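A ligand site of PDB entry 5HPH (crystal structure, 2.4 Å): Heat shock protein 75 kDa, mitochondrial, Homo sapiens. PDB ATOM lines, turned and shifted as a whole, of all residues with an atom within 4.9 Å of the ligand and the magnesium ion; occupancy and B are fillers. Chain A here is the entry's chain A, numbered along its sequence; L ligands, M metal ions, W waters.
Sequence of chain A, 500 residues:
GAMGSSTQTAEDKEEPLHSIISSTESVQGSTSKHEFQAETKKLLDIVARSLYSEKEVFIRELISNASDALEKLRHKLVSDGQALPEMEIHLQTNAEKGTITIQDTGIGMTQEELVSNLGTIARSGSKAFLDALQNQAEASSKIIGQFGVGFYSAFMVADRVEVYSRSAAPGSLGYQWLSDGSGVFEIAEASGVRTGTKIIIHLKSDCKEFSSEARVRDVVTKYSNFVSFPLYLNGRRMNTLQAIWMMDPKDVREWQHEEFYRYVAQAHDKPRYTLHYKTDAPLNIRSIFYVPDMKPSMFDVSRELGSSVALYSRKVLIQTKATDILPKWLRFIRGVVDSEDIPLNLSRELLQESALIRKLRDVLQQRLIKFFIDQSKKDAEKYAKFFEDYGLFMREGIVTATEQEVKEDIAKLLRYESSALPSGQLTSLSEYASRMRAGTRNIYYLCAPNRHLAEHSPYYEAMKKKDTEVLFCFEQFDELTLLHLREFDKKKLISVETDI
OG of Ser 124 sits at hydrogen-bond distance from O4 of the ligand (2.6 Å).
O1 of the ligand is in hydrogen-bond range of N of Gly 150 (2.7 Å).
The backbone NH of Gly 148 sits at hydrogen-bond distance from an oxygen (O1) of the ligand (3.1 Å).
The guanidinium group of Arg 348 is in salt-bridge range of an oxygen (O3) of the ligand, 2.8 Å away.
The backbone NH of Gln 146 is in hydrogen-bond range of an oxygen (O3) of the ligand (2.8 Å).
The backbone NH (N) of Gly 125 is in hydrogen-bond range of an oxygen (O11) of the ligand (2.8 Å).
The side-chain carboxylate (OD2) of Asp 104 sits at hydrogen-bond distance from a nitrogen (N4) of the ligand, at 2.9 Å.
N of Phe 151 is in hydrogen-bond range of O6 of the ligand, at 2.9 Å.
The backbone NH (N) of Val 149 is in hydrogen-bond range of an oxygen (O1) of the ligand (3.0 Å).
The backbone NH (N) of Phe 147 lies within hydrogen-bond range of an oxygen (O3) of the ligand (3.0 Å).
The backbone NH (N) of Ser 126 is in hydrogen-bond range of an oxygen (O11) of the ligand, at 3.1 Å.
The side-chain hydroxyl (OG1) of Thr 197 lies within hydrogen-bond range of a nitrogen (N5) of the ligand, 3.2 Å away.
The backbone carbonyl oxygen (O) of Glu 61 lies close to the side-chain amide nitrogen (ND2) of Asn 65 (3.5 Å).
O of Gln 146 sits close to OG of Ser 124, 3.5 Å away.
The guanidinium group (NH2) of Arg 348 sits close to the side-chain amide nitrogen (NE2) of Gln 146, 3.4 Å away.
N of Asp 104 lies within hydrogen-bond range of O of Thr 197.
The side-chain hydroxyl (OG) of Ser 126 sits at hydrogen-bond distance from the side-chain amino group (NZ) of Lys 72, at 3.0 Å.
OD1 of Asn 117 is in hydrogen-bond range of NE of Arg 123, at 2.6 Å.
O of Ala 69 is in hydrogen-bond range of N of Ile 107 (3.2 Å).
O of Leu 118 is in hydrogen-bond range of OH of Tyr 152, at 2.9 Å.
A nitrogen (N6) of the ligand lies close to the side-chain sulfur of Met 109 (3.7 Å).
Merely in contact with the ligand: Asn 117 (3.2 Å), Ala 69 (3.3 Å), Gly 145 (3.5 Å), Lys 72 (3.5 Å), Glu 61 (3.6 Å), Leu 118 (3.9 Å) and Arg 123 (3.9 Å).
Hydrophobic or aromatic side chains within 4 Å of the ligand: Ala 69, Met 109, Leu 118, Phe 147, Val 149 and Phe 151.
Within 4 Å of the ligand: Glu 61, Asn 65, Ala 69, Lys 72, Asp 104, Met 109, Asn 117, Leu 118, Arg 123, Ser 124, Gly 125, Ser 126, Gly 145, Gln 146, Phe 147, Gly 148, Val 149, Gly 150, Phe 151, Thr 197 and Arg 348.
Along chain A the residues within 4 Å of the ligand span positions 61 to 348.
O of Glu 61 touches the magnesium ion, 3.8 Å away.
Two residues have an atom within 4 Å of the magnesium ion: Glu 61 and Asn 65.
The nearest printed residue that does not touch the magnesium ion is Gly 150 (4.4 Å).
The magnesium ion is bound by the side-chain amide oxygen (OD1) of Asn 65 (2.0 Å).
The magnesium ion is bound by water W4, at 2.1 Å.
O2 of the ligand binds the magnesium ion (2.2 Å).
The magnesium ion is bound by an oxygen (O7) of the ligand.
An oxygen (O5) of the ligand binds the magnesium ion, 2.5 Å away.
The magnesium ion has five donor atoms within binding distance.
Water W1 lies within hydrogen-bond range of the side-chain carboxylate of Asp 104 (2.6 Å), the side-chain hydroxyl of Thr 197 (2.7 Å), a nitrogen (N5) of the ligand (2.7 Å) and the backbone NH of Gly 108 (2.9 Å).
Water W3 lies within hydrogen-bond range of the side-chain carboxylate of Glu 61, an oxygen (O1) of the ligand and the guanidinium group of Arg 348.
Water W2 lies within hydrogen-bond range of OG of Ser 126 (2.5 Å) and OD2 of Asp 68 (2.6 Å).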
ATOM      1  N   GLU A  61       4.696   4.512  19.020  1.00  0.00           N
ATOM      2  CA  GLU A  61       5.163   3.158  18.765  1.00  0.00           C
ATOM      3  C   GLU A  61       6.342   3.146  17.815  1.00  0.00           C
ATOM      4  O   GLU A  61       7.297   2.386  18.017  1.00  0.00           O
ATOM      5  CB  GLU A  61       4.027   2.289  18.220  1.00  0.00           C
ATOM      6  CG  GLU A  61       3.040   1.810  19.287  1.00  0.00           C
ATOM      7  CD  GLU A  61       3.746   1.356  20.581  1.00  0.00           C
ATOM      8  OE1 GLU A  61       3.755   2.123  21.568  1.00  0.00           O
ATOM      9  OE2 GLU A  61       4.284   0.219  20.592  1.00  0.00           O
ATOM     10  N   SER A  64       9.480   4.397  19.649  1.00  0.00           N
ATOM     11  CA  SER A  64      10.074   3.399  20.531  1.00  0.00           C
ATOM     12  C   SER A  64      10.850   2.352  19.735  1.00  0.00           C
ATOM     13  O   SER A  64      11.891   1.863  20.189  1.00  0.00           O
ATOM     14  CB  SER A  64       9.016   2.717  21.391  1.00  0.00           C
ATOM     15  OG  SER A  64       8.296   3.654  22.193  1.00  0.00           O
ATOM     16  N   ASN A  65      10.367   2.004  18.529  1.00  0.00           N
ATOM     17  CA  ASN A  65      11.077   1.055  17.690  1.00  0.00           C
ATOM     18  C   ASN A  65      12.384   1.638  17.159  1.00  0.00           C
ATOM     19  O   ASN A  65      13.420   0.960  17.145  1.00  0.00           O
ATOM     20  CB  ASN A  65      10.173   0.595  16.549  1.00  0.00           C
ATOM     21  CG  ASN A  65       9.078  -0.353  17.021  1.00  0.00           C
ATOM     22  OD1 ASN A  65       9.196  -0.947  18.079  1.00  0.00           O
ATOM     23  ND2 ASN A  65       8.020  -0.493  16.215  1.00  0.00           N
ATOM     24  N   ALA A  66      12.346   2.907  16.739  1.00  0.00           N
ATOM     25  CA  ALA A  66      13.562   3.630  16.381  1.00  0.00           C
ATOM     26  C   ALA A  66      14.539   3.656  17.545  1.00  0.00           C
ATOM     27  O   ALA A  66      15.715   3.305  17.397  1.00  0.00           O
ATOM     28  CB  ALA A  66      13.184   5.049  15.970  1.00  0.00           C
ATOM     29  N   ASP A  68      14.731   1.589  20.020  1.00  0.00           N
ATOM     30  CA  ASP A  68      15.231   0.240  20.279  1.00  0.00           C
ATOM     31  C   ASP A  68      16.280  -0.188  19.256  1.00  0.00           C
ATOM     32  O   ASP A  68      17.240  -0.892  19.599  1.00  0.00           O
ATOM     33  CB  ASP A  68      14.077  -0.759  20.259  1.00  0.00           C
ATOM     34  CG  ASP A  68      13.174  -0.648  21.470  1.00  0.00           C
ATOM     35  OD1 ASP A  68      13.583  -0.042  22.500  1.00  0.00           O
ATOM     36  OD2 ASP A  68      12.041  -1.196  21.362  1.00  0.00           O
ATOM     37  N   ALA A  69      16.090   0.203  17.991  1.00  0.00           N
ATOM     38  CA  ALA A  69      17.067  -0.102  16.950  1.00  0.00           C
ATOM     39  C   ALA A  69      18.403   0.562  17.264  1.00  0.00           C
ATOM     40  O   ALA A  69      19.458  -0.065  17.164  1.00  0.00           O
ATOM     41  CB  ALA A  69      16.526   0.383  15.605  1.00  0.00           C
ATOM     42  N   LYS A  72      20.084  -1.209  20.150  1.00  0.00           N
ATOM     43  CA  LYS A  72      20.773  -2.436  19.759  1.00  0.00           C
ATOM     44  C   LYS A  72      22.108  -2.130  19.069  1.00  0.00           C
ATOM     45  O   LYS A  72      23.144  -2.700  19.419  1.00  0.00           O
ATOM     46  CB  LYS A  72      19.896  -3.297  18.848  1.00  0.00           C
ATOM     47  CG  LYS A  72      18.613  -3.819  19.508  1.00  0.00           C
ATOM     48  CD  LYS A  72      17.725  -4.508  18.473  1.00  0.00           C
ATOM     49  CE  LYS A  72      16.436  -5.026  19.070  1.00  0.00           C
ATOM     50  NZ  LYS A  72      15.374  -5.090  17.999  1.00  0.00           N
ATOM     51  N   ASP A 104      15.575   6.062  11.265  1.00  0.00           N
ATOM     52  CA  ASP A 104      16.595   5.939  12.289  1.00  0.00           C
ATOM     53  C   ASP A 104      17.861   5.367  11.680  1.00  0.00           C
ATOM     54  O   ASP A 104      17.811   4.629  10.686  1.00  0.00           O
ATOM     55  CB  ASP A 104      16.132   5.058  13.487  1.00  0.00           C
ATOM     56  CG  ASP A 104      16.045   3.566  13.141  1.00  0.00           C
ATOM     57  OD1 ASP A 104      17.103   2.882  13.117  1.00  0.00           O
ATOM     58  OD2 ASP A 104      14.900   3.069  12.948  1.00  0.00           O
ATOM     59  N   ILE A 107      20.132  -0.215  14.063  1.00  0.00           N
ATOM     60  CA  ILE A 107      20.651  -1.518  13.631  1.00  0.00           C
ATOM     61  C   ILE A 107      20.098  -2.017  12.298  1.00  0.00           C
ATOM     62  O   ILE A 107      20.765  -2.813  11.617  1.00  0.00           O
ATOM     63  CB  ILE A 107      20.434  -2.578  14.735  1.00  0.00           C
ATOM     64  CG1 ILE A 107      21.233  -3.844  14.393  1.00  0.00           C
ATOM     65  CG2 ILE A 107      18.932  -2.891  14.945  1.00  0.00           C
ATOM     66  CD1 ILE A 107      21.868  -4.504  15.594  1.00  0.00           C
ATOM     67  N   GLY A 108      18.924  -1.564  11.875  1.00  0.00           N
ATOM     68  CA  GLY A 108      18.401  -2.011  10.581  1.00  0.00           C
ATOM     69  C   GLY A 108      18.005  -3.494  10.566  1.00  0.00           C
ATOM     70  O   GLY A 108      18.007  -4.201  11.582  1.00  0.00           O
ATOM     71  N   MET A 109      17.618  -3.947   9.375  1.00  0.00           N
ATOM     72  CA  MET A 109      17.077  -5.297   9.257  1.00  0.00           C
ATOM     73  C   MET A 109      17.569  -5.968   7.982  1.00  0.00           C
ATOM     74  O   MET A 109      17.431  -5.387   6.897  1.00  0.00           O
ATOM     75  CB  MET A 109      15.534  -5.286   9.297  1.00  0.00           C
ATOM     76  CG  MET A 109      14.906  -5.103  10.661  1.00  0.00           C
ATOM     77  SD  MET A 109      13.088  -5.090  10.683  1.00  0.00           S
ATOM     78  CE  MET A 109      12.751  -3.433  10.131  1.00  0.00           C
ATOM     79  N   ASN A 117      10.361 -10.163  11.624  1.00  0.00           N
ATOM     80  CA  ASN A 117       9.991  -9.234  12.680  1.00  0.00           C
ATOM     81  C   ASN A 117       8.799  -8.367  12.301  1.00  0.00           C
ATOM     82  O   ASN A 117       7.965  -8.070  13.156  1.00  0.00           O
ATOM     83  CB  ASN A 117      11.192  -8.354  13.046  1.00  0.00           C
ATOM     84  CG  ASN A 117      12.343  -9.137  13.611  1.00  0.00           C
ATOM     85  OD1 ASN A 117      12.152 -10.114  14.345  1.00  0.00           O
ATOM     86  ND2 ASN A 117      13.551  -8.720  13.287  1.00  0.00           N
ATOM     87  N   LEU A 118       8.737  -7.909  11.048  1.00  0.00           N
ATOM     88  CA  LEU A 118       7.521  -7.234  10.572  1.00  0.00           C
ATOM     89  C   LEU A 118       6.426  -8.204  10.134  1.00  0.00           C
ATOM     90  O   LEU A 118       5.249  -7.823  10.140  1.00  0.00           O
ATOM     91  CB  LEU A 118       7.853  -6.290   9.412  1.00  0.00           C
ATOM     92  CG  LEU A 118       8.864  -5.184   9.716  1.00  0.00           C
ATOM     93  CD1 LEU A 118       8.959  -4.195   8.528  1.00  0.00           C
ATOM     94  CD2 LEU A 118       8.483  -4.488  11.034  1.00  0.00           C
ATOM     95  N   ARG A 123       5.882 -11.483  16.917  1.00  0.00           N
ATOM     96  CA  ARG A 123       7.320 -11.724  16.914  1.00  0.00           C
ATOM     97  C   ARG A 123       8.034 -10.438  17.343  1.00  0.00           C
ATOM     98  O   ARG A 123       7.852  -9.369  16.736  1.00  0.00           O
ATOM     99  CB  ARG A 123       7.751 -12.193  15.529  1.00  0.00           C
ATOM    100  CG  ARG A 123       9.215 -11.972  15.167  1.00  0.00           C
ATOM    101  CD  ARG A 123      10.207 -12.677  16.096  1.00  0.00           C
ATOM    102  NE  ARG A 123      11.585 -12.270  15.771  1.00  0.00           N
ATOM    103  CZ  ARG A 123      12.689 -12.713  16.378  1.00  0.00           C
ATOM    104  NH1 ARG A 123      12.612 -13.580  17.372  1.00  0.00           N
ATOM    105  NH2 ARG A 123      13.868 -12.289  15.991  1.00  0.00           N
ATOM    106  N   SER A 124       8.816 -10.521  18.412  1.00  0.00           N
ATOM    107  CA  SER A 124       9.522  -9.356  18.932  1.00  0.00           C
ATOM    108  C   SER A 124      11.017  -9.650  18.900  1.00  0.00           C
ATOM    109  O   SER A 124      11.512 -10.453  19.695  1.00  0.00           O
ATOM    110  CB  SER A 124       9.056  -9.000  20.344  1.00  0.00           C
ATOM    111  OG  SER A 124       9.878  -8.013  20.958  1.00  0.00           O
ATOM    112  N   GLY A 125      11.723  -8.965  17.993  1.00  0.00           N
ATOM    113  CA  GLY A 125      13.180  -9.064  17.976  1.00  0.00           C
ATOM    114  C   GLY A 125      13.800  -8.410  19.187  1.00  0.00           C
ATOM    115  O   GLY A 125      14.772  -8.917  19.750  1.00  0.00           O
ATOM    116  N   SER A 126      13.231  -7.284  19.622  1.00  0.00           N
ATOM    117  CA  SER A 126      13.728  -6.609  20.820  1.00  0.00           C
ATOM    118  C   SER A 126      13.632  -7.514  22.049  1.00  0.00           C
ATOM    119  O   SER A 126      14.563  -7.578  22.854  1.00  0.00           O
ATOM    120  CB  SER A 126      12.957  -5.307  21.009  1.00  0.00           C
ATOM    121  OG  SER A 126      13.203  -4.406  19.922  1.00  0.00           O
ATOM    122  N   ILE A 144      12.444  -0.827  24.940  1.00  0.00           N
ATOM    123  CA  ILE A 144      11.009  -0.589  25.201  1.00  0.00           C
ATOM    124  C   ILE A 144      10.119  -1.757  24.736  1.00  0.00           C
ATOM    125  O   ILE A 144       9.153  -2.103  25.430  1.00  0.00           O
ATOM    126  CB  ILE A 144      10.605   0.744  24.554  1.00  0.00           C
ATOM    127  CG1 ILE A 144      11.549   1.859  25.083  1.00  0.00           C
ATOM    128  CG2 ILE A 144       9.098   1.070  24.784  1.00  0.00           C
ATOM    129  CD1 ILE A 144      11.775   3.030  24.116  1.00  0.00           C
ATOM    130  N   GLY A 145      10.426  -2.371  23.594  1.00  0.00           N
ATOM    131  CA  GLY A 145       9.491  -3.330  22.986  1.00  0.00           C
ATOM    132  C   GLY A 145       9.467  -4.696  23.668  1.00  0.00           C
ATOM    133  O   GLY A 145      10.492  -5.196  24.145  1.00  0.00           O
ATOM    134  N   GLN A 146       8.264  -5.256  23.790  1.00  0.00           N
ATOM    135  CA  GLN A 146       8.024  -6.612  24.318  1.00  0.00           C
ATOM    136  C   GLN A 146       7.056  -7.410  23.434  1.00  0.00           C
ATOM    137  O   GLN A 146       7.263  -8.597  23.194  1.00  0.00           O
ATOM    138  CB  GLN A 146       7.555  -6.582  25.768  1.00  0.00           C
ATOM    139  CG  GLN A 146       6.438  -5.621  26.086  1.00  0.00           C
ATOM    140  CD  GLN A 146       6.244  -5.448  27.580  1.00  0.00           C
ATOM    141  OE1 GLN A 146       6.373  -6.400  28.344  1.00  0.00           O
ATOM    142  NE2 GLN A 146       5.958  -4.221  28.007  1.00  0.00           N
ATOM    143  N   PHE A 147       5.877  -6.827  23.155  1.00  0.00           N
ATOM    144  CA  PHE A 147       4.721  -7.554  22.648  1.00  0.00           C
ATOM    145  C   PHE A 147       4.857  -8.035  21.209  1.00  0.00           C
ATOM    146  O   PHE A 147       4.227  -9.033  20.832  1.00  0.00           O
ATOM    147  CB  PHE A 147       3.484  -6.668  22.769  1.00  0.00           C
ATOM    148  CG  PHE A 147       3.211  -6.230  24.169  1.00  0.00           C
ATOM    149  CD1 PHE A 147       2.925  -7.166  25.162  1.00  0.00           C
ATOM    150  CD2 PHE A 147       3.245  -4.878  24.499  1.00  0.00           C
ATOM    151  CE1 PHE A 147       2.667  -6.768  26.469  1.00  0.00           C
ATOM    152  CE2 PHE A 147       2.981  -4.460  25.801  1.00  0.00           C
ATOM    153  CZ  PHE A 147       2.697  -5.411  26.777  1.00  0.00           C
ATOM    154  N   GLY A 148       5.587  -7.306  20.363  1.00  0.00           N
ATOM    155  CA  GLY A 148       5.663  -7.617  18.955  1.00  0.00           C
ATOM    156  C   GLY A 148       4.482  -7.159  18.110  1.00  0.00           C
ATOM    157  O   GLY A 148       4.297  -7.698  17.008  1.00  0.00           O
ATOM    158  N   VAL A 149       3.576  -6.346  18.645  1.00  0.00           N
ATOM    159  CA  VAL A 149       2.485  -5.796  17.838  1.00  0.00           C
ATOM    160  C   VAL A 149       2.606  -4.306  17.495  1.00  0.00           C
ATOM    161  O   VAL A 149       1.896  -3.860  16.584  1.00  0.00           O
ATOM    162  CB  VAL A 149       1.135  -6.056  18.517  1.00  0.00           C
ATOM    163  CG1 VAL A 149       1.019  -7.546  18.808  1.00  0.00           C
ATOM    164  CG2 VAL A 149       1.044  -5.248  19.814  1.00  0.00           C
ATOM    165  N   GLY A 150       3.520  -3.551  18.091  1.00  0.00           N
ATOM    166  CA  GLY A 150       3.368  -2.108  18.062  1.00  0.00           C
ATOM    167  C   GLY A 150       3.540  -1.497  16.676  1.00  0.00           C
ATOM    168  O   GLY A 150       2.978  -0.434  16.385  1.00  0.00           O
ATOM    169  N   PHE A 151       4.341  -2.129  15.820  1.00  0.00           N
ATOM    170  CA  PHE A 151       4.509  -1.595  14.474  1.00  0.00           C
ATOM    171  C   PHE A 151       3.201  -1.596  13.690  1.00  0.00           C
ATOM    172  O   PHE A 151       2.957  -0.691  12.887  1.00  0.00           O
ATOM    173  CB  PHE A 151       5.593  -2.400  13.728  1.00  0.00           C
ATOM    174  CG  PHE A 151       5.626  -2.146  12.256  1.00  0.00           C
ATOM    175  CD1 PHE A 151       6.308  -1.061  11.746  1.00  0.00           C
ATOM    176  CD2 PHE A 151       4.958  -2.994  11.380  1.00  0.00           C
ATOM    177  CE1 PHE A 151       6.333  -0.817  10.380  1.00  0.00           C
ATOM    178  CE2 PHE A 151       4.983  -2.750  10.014  1.00  0.00           C
ATOM    179  CZ  PHE A 151       5.665  -1.663   9.514  1.00  0.00           C
ATOM    180  N   TYR A 152       2.331  -2.590  13.933  1.00  0.00           N
ATOM    181  CA  TYR A 152       1.057  -2.681  13.222  1.00  0.00           C
ATOM    182  C   TYR A 152       0.133  -1.524  13.551  1.00  0.00           C
ATOM    183  O   TYR A 152      -0.791  -1.233  12.783  1.00  0.00           O
ATOM    184  CB  TYR A 152       0.372  -4.020  13.526  1.00  0.00           C
ATOM    185  CG  TYR A 152       1.312  -5.204  13.285  1.00  0.00           C
ATOM    186  CD1 TYR A 152       1.977  -5.362  12.069  1.00  0.00           C
ATOM    187  CD2 TYR A 152       1.571  -6.134  14.279  1.00  0.00           C
ATOM    188  CE1 TYR A 152       2.834  -6.442  11.835  1.00  0.00           C
ATOM    189  CE2 TYR A 152       2.421  -7.224  14.058  1.00  0.00           C
ATOM    190  CZ  TYR A 152       3.048  -7.363  12.838  1.00  0.00           C
ATOM    191  OH  TYR A 152       3.905  -8.436  12.634  1.00  0.00           O
ATOM    192  N   THR A 197      16.582   2.218   9.323  1.00  0.00           N
ATOM    193  CA  THR A 197      15.250   1.899   8.823  1.00  0.00           C
ATOM    194  C   THR A 197      14.502   3.199   8.559  1.00  0.00           C
ATOM    195  O   THR A 197      14.519   4.103   9.389  1.00  0.00           O
ATOM    196  CB  THR A 197      14.497   1.013   9.810  1.00  0.00           C
ATOM    197  OG1 THR A 197      15.285  -0.138  10.099  1.00  0.00           O
ATOM    198  CG2 THR A 197      13.174   0.572   9.236  1.00  0.00           C
ATOM    199  N   ILE A 199      10.671   4.409   7.547  1.00  0.00           N
ATOM    200  CA  ILE A 199       9.285   4.002   7.429  1.00  0.00           C
ATOM    201  C   ILE A 199       8.506   5.175   6.857  1.00  0.00           C
ATOM    202  O   ILE A 199       8.529   6.283   7.400  1.00  0.00           O
ATOM    203  CB  ILE A 199       8.700   3.557   8.770  1.00  0.00           C
ATOM    204  CG1 ILE A 199       9.542   2.421   9.363  1.00  0.00           C
ATOM    205  CG2 ILE A 199       7.250   3.170   8.596  1.00  0.00           C
ATOM    206  CD1 ILE A 199       9.136   2.027  10.761  1.00  0.00           C
ATOM    207  N   ARG A 348      -0.355  -0.230  26.273  1.00  0.00           N
ATOM    208  CA  ARG A 348       0.643   0.633  26.893  1.00  0.00           C
ATOM    209  C   ARG A 348       0.055   1.967  27.370  1.00  0.00           C
ATOM    210  O   ARG A 348       0.787   2.947  27.533  1.00  0.00           O
ATOM    211  CB  ARG A 348       1.819   0.866  25.935  1.00  0.00           C
ATOM    212  CG  ARG A 348       2.433  -0.429  25.407  1.00  0.00           C
ATOM    213  CD  ARG A 348       3.561  -0.167  24.360  1.00  0.00           C
ATOM    214  NE  ARG A 348       4.457  -1.319  24.318  1.00  0.00           N
ATOM    215  CZ  ARG A 348       5.491  -1.443  25.136  1.00  0.00           C
ATOM    216  NH1 ARG A 348       5.753  -0.472  25.998  1.00  0.00           N
ATOM    217  NH2 ARG A 348       6.277  -2.513  25.087  1.00  0.00           N
HETATM  218  P1  LIG L   1       6.014  -3.795  21.110  1.00  0.00           P
HETATM  219  O1  LIG L   1       4.753  -4.298  20.416  1.00  0.00           O
HETATM  220  O2  LIG L   1       6.574  -2.550  20.491  1.00  0.00           O
HETATM  221  O3  LIG L   1       6.088  -3.872  22.630  1.00  0.00           O
HETATM  222  P2  LIG L   1       8.137  -4.846  19.390  1.00  0.00           P
HETATM  223  O4  LIG L   1       9.084  -5.997  19.460  1.00  0.00           O
HETATM  224  O5  LIG L   1       8.667  -3.447  19.321  1.00  0.00           O
HETATM  225  N1  LIG L   1       7.139  -5.060  20.773  1.00  0.00           N
HETATM  226  P3  LIG L   1       6.934  -4.092  16.960  1.00  0.00           P
HETATM  227  O6  LIG L   1       5.770  -4.602  16.153  1.00  0.00           O
HETATM  228  O7  LIG L   1       6.946  -2.704  17.518  1.00  0.00           O
HETATM  229  O8  LIG L   1       7.180  -5.135  18.136  1.00  0.00           O
HETATM  230  O9  LIG L   1       8.294  -4.351  16.129  1.00  0.00           O
HETATM  231  C1  LIG L   1       8.512  -5.679  15.645  1.00  0.00           C
HETATM  232  C2  LIG L   1      10.002  -5.962  15.487  1.00  0.00           C
HETATM  233  O10 LIG L   1      10.485  -5.429  14.250  1.00  0.00           O
HETATM  234  C3  LIG L   1      10.870  -5.359  16.595  1.00  0.00           C
HETATM  235  O11 LIG L   1      11.027  -6.220  17.748  1.00  0.00           O
HETATM  236  C4  LIG L   1      12.175  -5.173  15.852  1.00  0.00           C
HETATM  237  O12 LIG L   1      12.880  -6.427  15.910  1.00  0.00           O
HETATM  238  C5  LIG L   1      11.778  -4.914  14.405  1.00  0.00           C
HETATM  239  N2  LIG L   1      11.719  -3.467  14.127  1.00  0.00           N
HETATM  240  C6  LIG L   1      10.648  -2.657  14.202  1.00  0.00           C
HETATM  241  N3  LIG L   1      10.972  -1.365  13.925  1.00  0.00           N
HETATM  242  C7  LIG L   1      12.286  -1.339  13.674  1.00  0.00           C
HETATM  243  C8  LIG L   1      13.294  -0.316  13.319  1.00  0.00           C
HETATM  244  N4  LIG L   1      12.956   0.982  13.163  1.00  0.00           N
HETATM  245  N5  LIG L   1      14.583  -0.731  13.155  1.00  0.00           N
HETATM  246  C9  LIG L   1      14.950  -2.024  13.288  1.00  0.00           C
HETATM  247  N6  LIG L   1      14.093  -3.005  13.611  1.00  0.00           N
HETATM  248  C10 LIG L   1      12.775  -2.722  13.808  1.00  0.00           C
HETATM  249 MG    MG M   1       7.552  -1.208  19.112  1.00  0.00          MG
HETATM  250  O   HOH W   1      16.849   0.408  12.229  1.00  0.00           O
HETATM  251  O   HOH W   2      11.553  -2.713  19.246  1.00  0.00           O
HETATM  252  O   HOH W   3       3.541  -2.059  21.609  1.00  0.00           O
HETATM  253  O   HOH W   4       8.983  -0.942  20.664  1.00  0.00           O
